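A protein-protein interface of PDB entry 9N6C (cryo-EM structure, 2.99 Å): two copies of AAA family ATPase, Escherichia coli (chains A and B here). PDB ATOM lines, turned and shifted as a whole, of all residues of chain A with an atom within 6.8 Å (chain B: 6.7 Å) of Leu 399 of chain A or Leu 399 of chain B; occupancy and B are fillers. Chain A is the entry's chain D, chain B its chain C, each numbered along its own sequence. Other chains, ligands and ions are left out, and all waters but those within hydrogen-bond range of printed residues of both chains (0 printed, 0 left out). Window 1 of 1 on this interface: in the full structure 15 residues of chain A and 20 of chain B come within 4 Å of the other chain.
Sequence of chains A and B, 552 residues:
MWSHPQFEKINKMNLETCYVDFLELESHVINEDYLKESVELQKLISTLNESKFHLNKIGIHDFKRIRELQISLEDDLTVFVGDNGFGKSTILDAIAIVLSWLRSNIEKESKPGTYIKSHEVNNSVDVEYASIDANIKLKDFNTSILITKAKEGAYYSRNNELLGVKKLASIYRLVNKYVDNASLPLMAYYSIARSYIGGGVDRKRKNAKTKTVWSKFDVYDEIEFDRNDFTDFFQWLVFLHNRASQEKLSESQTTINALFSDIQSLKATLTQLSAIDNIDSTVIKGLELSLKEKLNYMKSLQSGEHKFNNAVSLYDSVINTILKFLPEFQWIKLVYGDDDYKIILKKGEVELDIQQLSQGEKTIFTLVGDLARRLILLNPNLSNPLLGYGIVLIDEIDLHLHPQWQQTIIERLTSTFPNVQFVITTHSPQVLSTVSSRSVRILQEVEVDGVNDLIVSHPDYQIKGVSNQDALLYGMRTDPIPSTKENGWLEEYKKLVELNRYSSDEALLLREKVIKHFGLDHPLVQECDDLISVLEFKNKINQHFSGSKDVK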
ATOM      1  N   SER A 191      22.655 -17.149   5.391  1.00  0.00           N
ATOM      2  CA  SER A 191      23.216 -17.048   4.057  1.00  0.00           C
ATOM      3  C   SER A 191      23.768 -18.400   3.608  1.00  0.00           C
ATOM      4  O   SER A 191      23.603 -19.421   4.281  1.00  0.00           O
ATOM      5  CB  SER A 191      24.287 -15.959   4.031  1.00  0.00           C
ATOM      6  OG  SER A 191      25.485 -16.414   4.634  1.00  0.00           O
ATOM      7  N   ILE A 192      24.427 -18.410   2.447  1.00  0.00           N
ATOM      8  CA  ILE A 192      25.041 -19.631   1.936  1.00  0.00           C
ATOM      9  C   ILE A 192      26.178 -20.091   2.841  1.00  0.00           C
ATOM     10  O   ILE A 192      26.477 -21.289   2.915  1.00  0.00           O
ATOM     11  CB  ILE A 192      25.514 -19.407   0.488  1.00  0.00           C
ATOM     12  CG1 ILE A 192      24.321 -19.089  -0.408  1.00  0.00           C
ATOM     13  CG2 ILE A 192      26.240 -20.626  -0.048  1.00  0.00           C
ATOM     14  CD1 ILE A 192      23.263 -20.166  -0.403  1.00  0.00           C
ATOM     15  N   ARG A 194      26.131 -20.728   5.651  1.00  0.00           N
ATOM     16  CA  ARG A 194      25.609 -21.691   6.615  1.00  0.00           C
ATOM     17  C   ARG A 194      26.320 -23.033   6.510  1.00  0.00           C
ATOM     18  O   ARG A 194      26.378 -23.786   7.488  1.00  0.00           O
ATOM     19  CB  ARG A 194      24.105 -21.853   6.391  1.00  0.00           C
ATOM     20  CG  ARG A 194      23.397 -22.795   7.338  1.00  0.00           C
ATOM     21  CD  ARG A 194      21.885 -22.709   7.163  1.00  0.00           C
ATOM     22  NE  ARG A 194      21.435 -23.152   5.847  1.00  0.00           N
ATOM     23  CZ  ARG A 194      21.150 -22.343   4.836  1.00  0.00           C
ATOM     24  NH1 ARG A 194      21.262 -21.030   4.948  1.00  0.00           N
ATOM     25  NH2 ARG A 194      20.736 -22.862   3.686  1.00  0.00           N
ATOM     26  N   SER A 195      26.874 -23.344   5.343  1.00  0.00           N
ATOM     27  CA  SER A 195      27.587 -24.591   5.107  1.00  0.00           C
ATOM     28  C   SER A 195      29.009 -24.496   5.664  1.00  0.00           C
ATOM     29  O   SER A 195      29.333 -23.623   6.473  1.00  0.00           O
ATOM     30  CB  SER A 195      27.582 -24.929   3.619  1.00  0.00           C
ATOM     31  OG  SER A 195      26.303 -24.708   3.052  1.00  0.00           O
ATOM     32  N   GLN A 359      25.364 -34.605   6.318  1.00  0.00           N
ATOM     33  CA  GLN A 359      25.296 -33.157   6.138  1.00  0.00           C
ATOM     34  C   GLN A 359      23.865 -32.637   6.194  1.00  0.00           C
ATOM     35  O   GLN A 359      23.618 -31.542   6.726  1.00  0.00           O
ATOM     36  CB  GLN A 359      25.941 -32.774   4.809  1.00  0.00           C
ATOM     37  CG  GLN A 359      26.381 -31.329   4.723  1.00  0.00           C
ATOM     38  CD  GLN A 359      27.756 -31.110   5.313  1.00  0.00           C
ATOM     39  OE1 GLN A 359      28.567 -32.032   5.381  1.00  0.00           O
ATOM     40  NE2 GLN A 359      28.028 -29.885   5.741  1.00  0.00           N
ATOM     41  N   GLY A 360      22.907 -33.429   5.709  1.00  0.00           N
ATOM     42  CA  GLY A 360      21.526 -32.983   5.711  1.00  0.00           C
ATOM     43  C   GLY A 360      20.966 -32.803   7.105  1.00  0.00           C
ATOM     44  O   GLY A 360      20.301 -31.804   7.388  1.00  0.00           O
ATOM     45  N   THR A 363      22.564 -29.717   8.888  1.00  0.00           N
ATOM     46  CA  THR A 363      22.075 -28.391   8.536  1.00  0.00           C
ATOM     47  C   THR A 363      20.811 -28.071   9.320  1.00  0.00           C
ATOM     48  O   THR A 363      20.680 -26.978   9.892  1.00  0.00           O
ATOM     49  CB  THR A 363      21.817 -28.309   7.033  1.00  0.00           C
ATOM     50  OG1 THR A 363      23.066 -28.259   6.333  1.00  0.00           O
ATOM     51  CG2 THR A 363      21.007 -27.070   6.696  1.00  0.00           C
ATOM     52  N   ASP A 395      18.054 -18.074   2.461  1.00  0.00           N
ATOM     53  CA  ASP A 395      18.454 -18.208   1.068  1.00  0.00           C
ATOM     54  C   ASP A 395      18.731 -19.674   0.768  1.00  0.00           C
ATOM     55  O   ASP A 395      19.514 -20.316   1.474  1.00  0.00           O
ATOM     56  CB  ASP A 395      19.692 -17.363   0.762  1.00  0.00           C
ATOM     57  CG  ASP A 395      19.923 -17.188  -0.726  1.00  0.00           C
ATOM     58  OD1 ASP A 395      19.088 -17.663  -1.522  1.00  0.00           O
ATOM     59  OD2 ASP A 395      20.943 -16.573  -1.101  1.00  0.00           O
ATOM     60  N   GLU A 396      18.093 -20.192  -0.284  1.00  0.00           N
ATOM     61  CA  GLU A 396      18.316 -21.557  -0.761  1.00  0.00           C
ATOM     62  C   GLU A 396      18.052 -22.575   0.351  1.00  0.00           C
ATOM     63  O   GLU A 396      18.944 -23.291   0.806  1.00  0.00           O
ATOM     64  CB  GLU A 396      19.728 -21.712  -1.333  1.00  0.00           C
ATOM     65  N   ILE A 397      16.792 -22.612   0.792  1.00  0.00           N
ATOM     66  CA  ILE A 397      16.387 -23.499   1.878  1.00  0.00           C
ATOM     67  C   ILE A 397      16.563 -24.966   1.500  1.00  0.00           C
ATOM     68  O   ILE A 397      16.649 -25.829   2.380  1.00  0.00           O
ATOM     69  CB  ILE A 397      14.929 -23.178   2.275  1.00  0.00           C
ATOM     70  CG1 ILE A 397      14.355 -24.210   3.243  1.00  0.00           C
ATOM     71  CG2 ILE A 397      14.059 -23.133   1.051  1.00  0.00           C
ATOM     72  CD1 ILE A 397      13.075 -23.769   3.903  1.00  0.00           C
ATOM     73  N   ASP A 398      16.688 -25.267   0.209  1.00  0.00           N
ATOM     74  CA  ASP A 398      16.704 -26.640  -0.290  1.00  0.00           C
ATOM     75  C   ASP A 398      18.121 -27.162  -0.485  1.00  0.00           C
ATOM     76  O   ASP A 398      18.397 -27.891  -1.441  1.00  0.00           O
ATOM     77  CB  ASP A 398      15.913 -26.744  -1.588  1.00  0.00           C
ATOM     78  CG  ASP A 398      16.302 -25.686  -2.594  1.00  0.00           C
ATOM     79  OD1 ASP A 398      15.833 -24.538  -2.459  1.00  0.00           O
ATOM     80  OD2 ASP A 398      17.077 -26.001  -3.518  1.00  0.00           O
ATOM     81  N   LEU A 399      19.040 -26.801   0.406  1.00  0.00           N
ATOM     82  CA  LEU A 399      20.413 -27.284   0.346  1.00  0.00           C
ATOM     83  C   LEU A 399      20.517 -28.610   1.089  1.00  0.00           C
ATOM     84  O   LEU A 399      20.205 -28.686   2.283  1.00  0.00           O
ATOM     85  CB  LEU A 399      21.369 -26.260   0.952  1.00  0.00           C
ATOM     86  CG  LEU A 399      22.111 -25.328  -0.003  1.00  0.00           C
ATOM     87  CD1 LEU A 399      23.403 -24.852   0.632  1.00  0.00           C
ATOM     88  CD2 LEU A 399      22.389 -26.021  -1.324  1.00  0.00           C
ATOM     89  N   HIS A 400      20.958 -29.650   0.378  1.00  0.00           N
ATOM     90  CA  HIS A 400      21.195 -30.977   0.948  1.00  0.00           C
ATOM     91  C   HIS A 400      19.924 -31.560   1.565  1.00  0.00           C
ATOM     92  O   HIS A 400      19.904 -31.967   2.728  1.00  0.00           O
ATOM     93  CB  HIS A 400      22.322 -30.939   1.983  1.00  0.00           C
ATOM     94  CG  HIS A 400      23.532 -30.178   1.542  1.00  0.00           C
ATOM     95  ND1 HIS A 400      24.270 -29.397   2.404  1.00  0.00           N
ATOM     96  CD2 HIS A 400      24.142 -30.088   0.338  1.00  0.00           C
ATOM     97  CE1 HIS A 400      25.279 -28.853   1.748  1.00  0.00           C
ATOM     98  NE2 HIS A 400      25.223 -29.255   0.492  1.00  0.00           N
ATOM     99  N   LEU A 401      18.853 -31.604   0.776  1.00  0.00           N
ATOM    100  CA  LEU A 401      17.596 -32.189   1.223  1.00  0.00           C
ATOM    101  C   LEU A 401      16.975 -32.992   0.091  1.00  0.00           C
ATOM    102  O   LEU A 401      16.905 -32.509  -1.042  1.00  0.00           O
ATOM    103  CB  LEU A 401      16.615 -31.106   1.692  1.00  0.00           C
ATOM    104  CG  LEU A 401      17.040 -30.166   2.821  1.00  0.00           C
ATOM    105  CD1 LEU A 401      16.053 -29.024   2.958  1.00  0.00           C
ATOM    106  CD2 LEU A 401      17.158 -30.918   4.128  1.00  0.00           C
ATOM    107  N   GLN A 406      11.772 -31.961   1.362  1.00  0.00           N
ATOM    108  CA  GLN A 406      11.441 -30.678   0.760  1.00  0.00           C
ATOM    109  C   GLN A 406       9.942 -30.434   0.725  1.00  0.00           C
ATOM    110  O   GLN A 406       9.517 -29.279   0.627  1.00  0.00           O
ATOM    111  CB  GLN A 406      12.011 -30.600  -0.654  1.00  0.00           C
ATOM    112  CG  GLN A 406      13.518 -30.461  -0.702  1.00  0.00           C
ATOM    113  CD  GLN A 406      14.067 -30.545  -2.111  1.00  0.00           C
ATOM    114  OE1 GLN A 406      13.345 -30.338  -3.084  1.00  0.00           O
ATOM    115  NE2 GLN A 406      15.352 -30.853  -2.226  1.00  0.00           N
ATOM    116  N   HIS A 427      14.555 -22.296  -6.074  1.00  0.00           N
ATOM    117  CA  HIS A 427      14.456 -22.540  -7.507  1.00  0.00           C
ATOM    118  C   HIS A 427      13.978 -23.953  -7.827  1.00  0.00           C
ATOM    119  O   HIS A 427      13.942 -24.322  -9.007  1.00  0.00           O
ATOM    120  CB  HIS A 427      15.796 -22.270  -8.213  1.00  0.00           C
ATOM    121  CG  HIS A 427      16.885 -23.231  -7.850  1.00  0.00           C
ATOM    122  ND1 HIS A 427      17.939 -22.885  -7.032  1.00  0.00           N
ATOM    123  CD2 HIS A 427      17.096 -24.519  -8.209  1.00  0.00           C
ATOM    124  CE1 HIS A 427      18.747 -23.921  -6.896  1.00  0.00           C
ATOM    125  NE2 HIS A 427      18.257 -24.926  -7.600  1.00  0.00           N
ATOM    126  N   SER B 191      35.033 -33.155  -3.445  1.00  0.00           N
ATOM    127  CA  SER B 191      34.161 -33.402  -2.305  1.00  0.00           C
ATOM    128  C   SER B 191      33.100 -32.310  -2.216  1.00  0.00           C
ATOM    129  O   SER B 191      32.976 -31.449  -3.091  1.00  0.00           O
ATOM    130  CB  SER B 191      34.985 -33.499  -1.026  1.00  0.00           C
ATOM    131  OG  SER B 191      35.741 -32.319  -0.826  1.00  0.00           O
ATOM    132  N   ILE B 192      32.312 -32.339  -1.139  1.00  0.00           N
ATOM    133  CA  ILE B 192      31.266 -31.341  -0.939  1.00  0.00           C
ATOM    134  C   ILE B 192      31.819 -30.010  -0.460  1.00  0.00           C
ATOM    135  O   ILE B 192      31.082 -29.017  -0.428  1.00  0.00           O
ATOM    136  CB  ILE B 192      30.218 -31.863   0.062  1.00  0.00           C
ATOM    137  CG1 ILE B 192      28.873 -31.175  -0.154  1.00  0.00           C
ATOM    138  CG2 ILE B 192      30.698 -31.658   1.486  1.00  0.00           C
ATOM    139  CD1 ILE B 192      28.005 -31.859  -1.180  1.00  0.00           C
ATOM    140  N   ARG B 194      33.858 -28.004  -1.915  1.00  0.00           N
ATOM    141  CA  ARG B 194      34.382 -27.196  -3.006  1.00  0.00           C
ATOM    142  C   ARG B 194      33.633 -25.884  -3.181  1.00  0.00           C
ATOM    143  O   ARG B 194      34.024 -25.072  -4.025  1.00  0.00           O
ATOM    144  CB  ARG B 194      34.351 -27.990  -4.315  1.00  0.00           C
ATOM    145  CG  ARG B 194      32.963 -28.207  -4.881  1.00  0.00           C
ATOM    146  CD  ARG B 194      33.028 -28.948  -6.204  1.00  0.00           C
ATOM    147  NE  ARG B 194      31.707 -29.180  -6.777  1.00  0.00           N
ATOM    148  CZ  ARG B 194      30.854 -30.099  -6.348  1.00  0.00           C
ATOM    149  NH1 ARG B 194      31.144 -30.892  -5.331  1.00  0.00           N
ATOM    150  NH2 ARG B 194      29.680 -30.227  -6.956  1.00  0.00           N
ATOM    151  N   SER B 195      32.565 -25.658  -2.415  1.00  0.00           N
ATOM    152  CA  SER B 195      31.837 -24.400  -2.496  1.00  0.00           C
ATOM    153  C   SER B 195      32.507 -23.291  -1.697  1.00  0.00           C
ATOM    154  O   SER B 195      32.245 -22.111  -1.957  1.00  0.00           O
ATOM    155  CB  SER B 195      30.401 -24.591  -2.009  1.00  0.00           C
ATOM    156  OG  SER B 195      30.374 -24.968  -0.644  1.00  0.00           O
ATOM    157  N   GLN B 359      26.879 -17.792  -7.795  1.00  0.00           N
ATOM    158  CA  GLN B 359      27.516 -18.968  -7.207  1.00  0.00           C
ATOM    159  C   GLN B 359      27.582 -20.130  -8.195  1.00  0.00           C
ATOM    160  O   GLN B 359      28.611 -20.821  -8.298  1.00  0.00           O
ATOM    161  CB  GLN B 359      26.757 -19.377  -5.945  1.00  0.00           C
ATOM    162  CG  GLN B 359      27.381 -20.512  -5.163  1.00  0.00           C
ATOM    163  CD  GLN B 359      28.534 -20.064  -4.286  1.00  0.00           C
ATOM    164  OE1 GLN B 359      29.368 -19.259  -4.696  1.00  0.00           O
ATOM    165  NE2 GLN B 359      28.582 -20.584  -3.068  1.00  0.00           N
ATOM    166  N   GLY B 360      26.513 -20.323  -8.970  1.00  0.00           N
ATOM    167  CA  GLY B 360      26.478 -21.441  -9.896  1.00  0.00           C
ATOM    168  C   GLY B 360      27.531 -21.333 -10.977  1.00  0.00           C
ATOM    169  O   GLY B 360      28.184 -22.322 -11.316  1.00  0.00           O
ATOM    170  N   THR B 363      30.988 -22.203  -9.641  1.00  0.00           N
ATOM    171  CA  THR B 363      31.278 -23.613  -9.408  1.00  0.00           C
ATOM    172  C   THR B 363      31.738 -24.290 -10.696  1.00  0.00           C
ATOM    173  O   THR B 363      32.741 -25.022 -10.705  1.00  0.00           O
ATOM    174  CB  THR B 363      30.044 -24.312  -8.838  1.00  0.00           C
ATOM    175  OG1 THR B 363      29.945 -24.039  -7.435  1.00  0.00           O
ATOM    176  CG2 THR B 363      30.131 -25.812  -9.045  1.00  0.00           C
ATOM    177  N   ASP B 395      30.793 -35.648  -6.135  1.00  0.00           N
ATOM    178  CA  ASP B 395      29.741 -35.824  -5.143  1.00  0.00           C
ATOM    179  C   ASP B 395      28.717 -34.707  -5.278  1.00  0.00           C
ATOM    180  O   ASP B 395      29.078 -33.527  -5.249  1.00  0.00           O
ATOM    181  CB  ASP B 395      30.321 -35.839  -3.728  1.00  0.00           C
ATOM    182  CG  ASP B 395      29.321 -36.311  -2.692  1.00  0.00           C
ATOM    183  OD1 ASP B 395      28.183 -36.655  -3.070  1.00  0.00           O
ATOM    184  OD2 ASP B 395      29.676 -36.342  -1.497  1.00  0.00           O
ATOM    185  N   GLU B 396      27.443 -35.084  -5.416  1.00  0.00           N
ATOM    186  CA  GLU B 396      26.323 -34.143  -5.470  1.00  0.00           C
ATOM    187  C   GLU B 396      26.498 -33.141  -6.616  1.00  0.00           C
ATOM    188  O   GLU B 396      26.678 -31.940  -6.422  1.00  0.00           O
ATOM    189  CB  GLU B 396      26.146 -33.426  -4.127  1.00  0.00           C
ATOM    190  CG  GLU B 396      25.697 -34.338  -3.005  1.00  0.00           C
ATOM    191  CD  GLU B 396      24.485 -33.803  -2.272  1.00  0.00           C
ATOM    192  OE1 GLU B 396      23.355 -34.024  -2.752  1.00  0.00           O
ATOM    193  OE2 GLU B 396      24.663 -33.164  -1.215  1.00  0.00           O
ATOM    194  N   ILE B 397      26.448 -33.693  -7.831  1.00  0.00           N
ATOM    195  CA  ILE B 397      26.659 -32.910  -9.044  1.00  0.00           C
ATOM    196  C   ILE B 397      25.631 -31.795  -9.208  1.00  0.00           C
ATOM    197  O   ILE B 397      25.866 -30.846  -9.962  1.00  0.00           O
ATOM    198  CB  ILE B 397      26.651 -33.857 -10.264  1.00  0.00           C
ATOM    199  CG1 ILE B 397      27.083 -33.126 -11.535  1.00  0.00           C
ATOM    200  CG2 ILE B 397      25.279 -34.470 -10.451  1.00  0.00           C
ATOM    201  CD1 ILE B 397      28.569 -33.149 -11.776  1.00  0.00           C
ATOM    202  N   ASP B 398      24.508 -31.862  -8.495  1.00  0.00           N
ATOM    203  CA  ASP B 398      23.398 -30.928  -8.687  1.00  0.00           C
ATOM    204  C   ASP B 398      23.415 -29.781  -7.684  1.00  0.00           C
ATOM    205  O   ASP B 398      22.359 -29.326  -7.239  1.00  0.00           O
ATOM    206  CB  ASP B 398      22.069 -31.674  -8.628  1.00  0.00           C
ATOM    207  CG  ASP B 398      21.951 -32.567  -7.411  1.00  0.00           C
ATOM    208  OD1 ASP B 398      22.229 -32.097  -6.290  1.00  0.00           O
ATOM    209  OD2 ASP B 398      21.580 -33.746  -7.576  1.00  0.00           O
ATOM    210  N   LEU B 399      24.593 -29.297  -7.306  1.00  0.00           N
ATOM    211  CA  LEU B 399      24.710 -28.203  -6.351  1.00  0.00           C
ATOM    212  C   LEU B 399      24.664 -26.863  -7.077  1.00  0.00           C
ATOM    213  O   LEU B 399      25.423 -26.639  -8.024  1.00  0.00           O
ATOM    214  CB  LEU B 399      26.010 -28.317  -5.557  1.00  0.00           C
ATOM    215  CG  LEU B 399      25.923 -28.869  -4.134  1.00  0.00           C
ATOM    216  CD1 LEU B 399      27.105 -28.384  -3.312  1.00  0.00           C
ATOM    217  CD2 LEU B 399      24.612 -28.479  -3.475  1.00  0.00           C
ATOM    218  N   HIS B 400      23.771 -25.980  -6.626  1.00  0.00           N
ATOM    219  CA  HIS B 400      23.667 -24.611  -7.139  1.00  0.00           C
ATOM    220  C   HIS B 400      23.385 -24.576  -8.640  1.00  0.00           C
ATOM    221  O   HIS B 400      23.869 -23.699  -9.356  1.00  0.00           O
ATOM    222  CB  HIS B 400      24.929 -23.806  -6.821  1.00  0.00           C
ATOM    223  CG  HIS B 400      25.300 -23.801  -5.372  1.00  0.00           C
ATOM    224  ND1 HIS B 400      24.363 -23.758  -4.363  1.00  0.00           N
ATOM    225  CD2 HIS B 400      26.509 -23.826  -4.763  1.00  0.00           C
ATOM    226  CE1 HIS B 400      24.979 -23.760  -3.194  1.00  0.00           C
ATOM    227  NE2 HIS B 400      26.281 -23.802  -3.409  1.00  0.00           N
ATOM    228  N   LEU B 401      22.590 -25.525  -9.125  1.00  0.00           N
ATOM    229  CA  LEU B 401      22.216 -25.575 -10.532  1.00  0.00           C
ATOM    230  C   LEU B 401      20.701 -25.631 -10.653  1.00  0.00           C
ATOM    231  O   LEU B 401      20.054 -26.442  -9.984  1.00  0.00           O
ATOM    232  CB  LEU B 401      22.843 -26.784 -11.231  1.00  0.00           C
ATOM    233  CG  LEU B 401      24.354 -26.957 -11.098  1.00  0.00           C
ATOM    234  CD1 LEU B 401      24.817 -28.185 -11.858  1.00  0.00           C
ATOM    235  CD2 LEU B 401      25.081 -25.723 -11.588  1.00  0.00           C
ATOM    236  N   HIS B 402      20.138 -24.775 -11.502  1.00  0.00           N
ATOM    237  CA  HIS B 402      18.710 -24.817 -11.763  1.00  0.00           C
ATOM    238  C   HIS B 402      18.379 -25.996 -12.674  1.00  0.00           C
ATOM    239  O   HIS B 402      19.261 -26.539 -13.344  1.00  0.00           O
ATOM    240  CB  HIS B 402      18.238 -23.495 -12.369  1.00  0.00           C
ATOM    241  CG  HIS B 402      19.011 -23.055 -13.570  1.00  0.00           C
ATOM    242  ND1 HIS B 402      20.304 -22.587 -13.495  1.00  0.00           N
ATOM    243  CD2 HIS B 402      18.659 -22.980 -14.875  1.00  0.00           C
ATOM    244  CE1 HIS B 402      20.722 -22.259 -14.705  1.00  0.00           C
ATOM    245  NE2 HIS B 402      19.743 -22.488 -15.560  1.00  0.00           N
ATOM    246  N   GLN B 406      20.551 -28.895 -15.118  1.00  0.00           N
ATOM    247  CA  GLN B 406      20.734 -30.219 -14.535  1.00  0.00           C
ATOM    248  C   GLN B 406      20.594 -31.323 -15.573  1.00  0.00           C
ATOM    249  O   GLN B 406      21.152 -32.411 -15.396  1.00  0.00           O
ATOM    250  CB  GLN B 406      19.734 -30.439 -13.402  1.00  0.00           C
ATOM    251  CG  GLN B 406      20.102 -29.747 -12.106  1.00  0.00           C
ATOM    252  CD  GLN B 406      19.181 -30.124 -10.965  1.00  0.00           C
ATOM    253  OE1 GLN B 406      18.455 -31.112 -11.042  1.00  0.00           O
ATOM    254  NE2 GLN B 406      19.203 -29.334  -9.902  1.00  0.00           N
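The guanidinium group (NH2) of Arg 194 of chain B lies within hydrogen-bond range of the backbone carbonyl oxygen (O) of Glu 396 of chain B (3.5 Å).
The side-chain hydroxyl (OG) of Ser 195 of chain A is in hydrogen-bond range of the backbone carbonyl oxygen (O) of Ile 192 of chain A, 3.4 Å away.
The side-chain amide nitrogen (NE2) of Gln 406 of chain B is in hydrogen-bond range of the backbone carbonyl oxygen (O) of Leu 401 of chain B, at 3.0 Å.
Of the 16 printed residues of chain B, 6 touch a printed residue of chain A.
Of the 16 printed residues of chain A, 4 touch a printed residue of chain B.
Hydrophobic or aromatic side chains of chain A that line the printed part of chain B: Ile 192, Leu 399, His 400 and His 427.
Among the printed residues, no Asp or Glu carboxylate lies within 4 Å of a Lys or Arg side-chain nitrogen of the other chain.
The backbone carbonyl oxygen (O) of Leu 401 of chain B is in hydrogen-bond range of a ring nitrogen (NE2) of His 427 of chain A, at 3.3 Å.
Ile 192 of chain A touches Gln 359 of chain B, but with the chains exchanged Gln 359 of chain A does not touch Ile 192 of chain B (4.5 Å).
Leu 399 of chain B touches its own counterpart, Leu 399 of chain A.
Leu 399 of chain A touches His 400 of chain B, but with the chains exchanged His 400 of chain A does not touch Leu 399 of chain B (4.1 Å).
His 400 of chain A touches Glu 396 of chain B, but with the chains exchanged Glu 396 of chain A does not touch His 400 of chain B (5.9 Å).
Leu 399 of chain B touches just one residue of chain A: Leu 399.
Of the printed residues of chain B, Ile 192 of chain A touches Gln 359 (3.8 Å).
Of the printed residues of chain A, Leu 401 of chain B touches His 427.
Of the printed residues of chain B, His 427 of chain A touches Leu 401 (3.3 Å) and His 402 (3.9 Å).
Printed residues of chain A within 4 Å of Gln 359 of chain B: Ile 192 (3.8 Å).
Gly 360 of chain B touches none of the printed residues of chain A.
The nearest printed residue of chain A that does not touch Gln 359 of chain B is Leu 399 of chain A (7.7 Å).
Among the printed residues, pairs that only touch across the chains: Ile 192 of chain A with Gln 359 of chain B (3.8 Å), Leu 399 of chain A with Leu 399 of chain B (3.95 Å), Leu 399 of chain A with His 400 of chain B (3.9 Å), His 400 of chain A with Glu 396 of chain B (3.5 Å) and His 427 of chain A with His 402 of chain B (3.9 Å).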
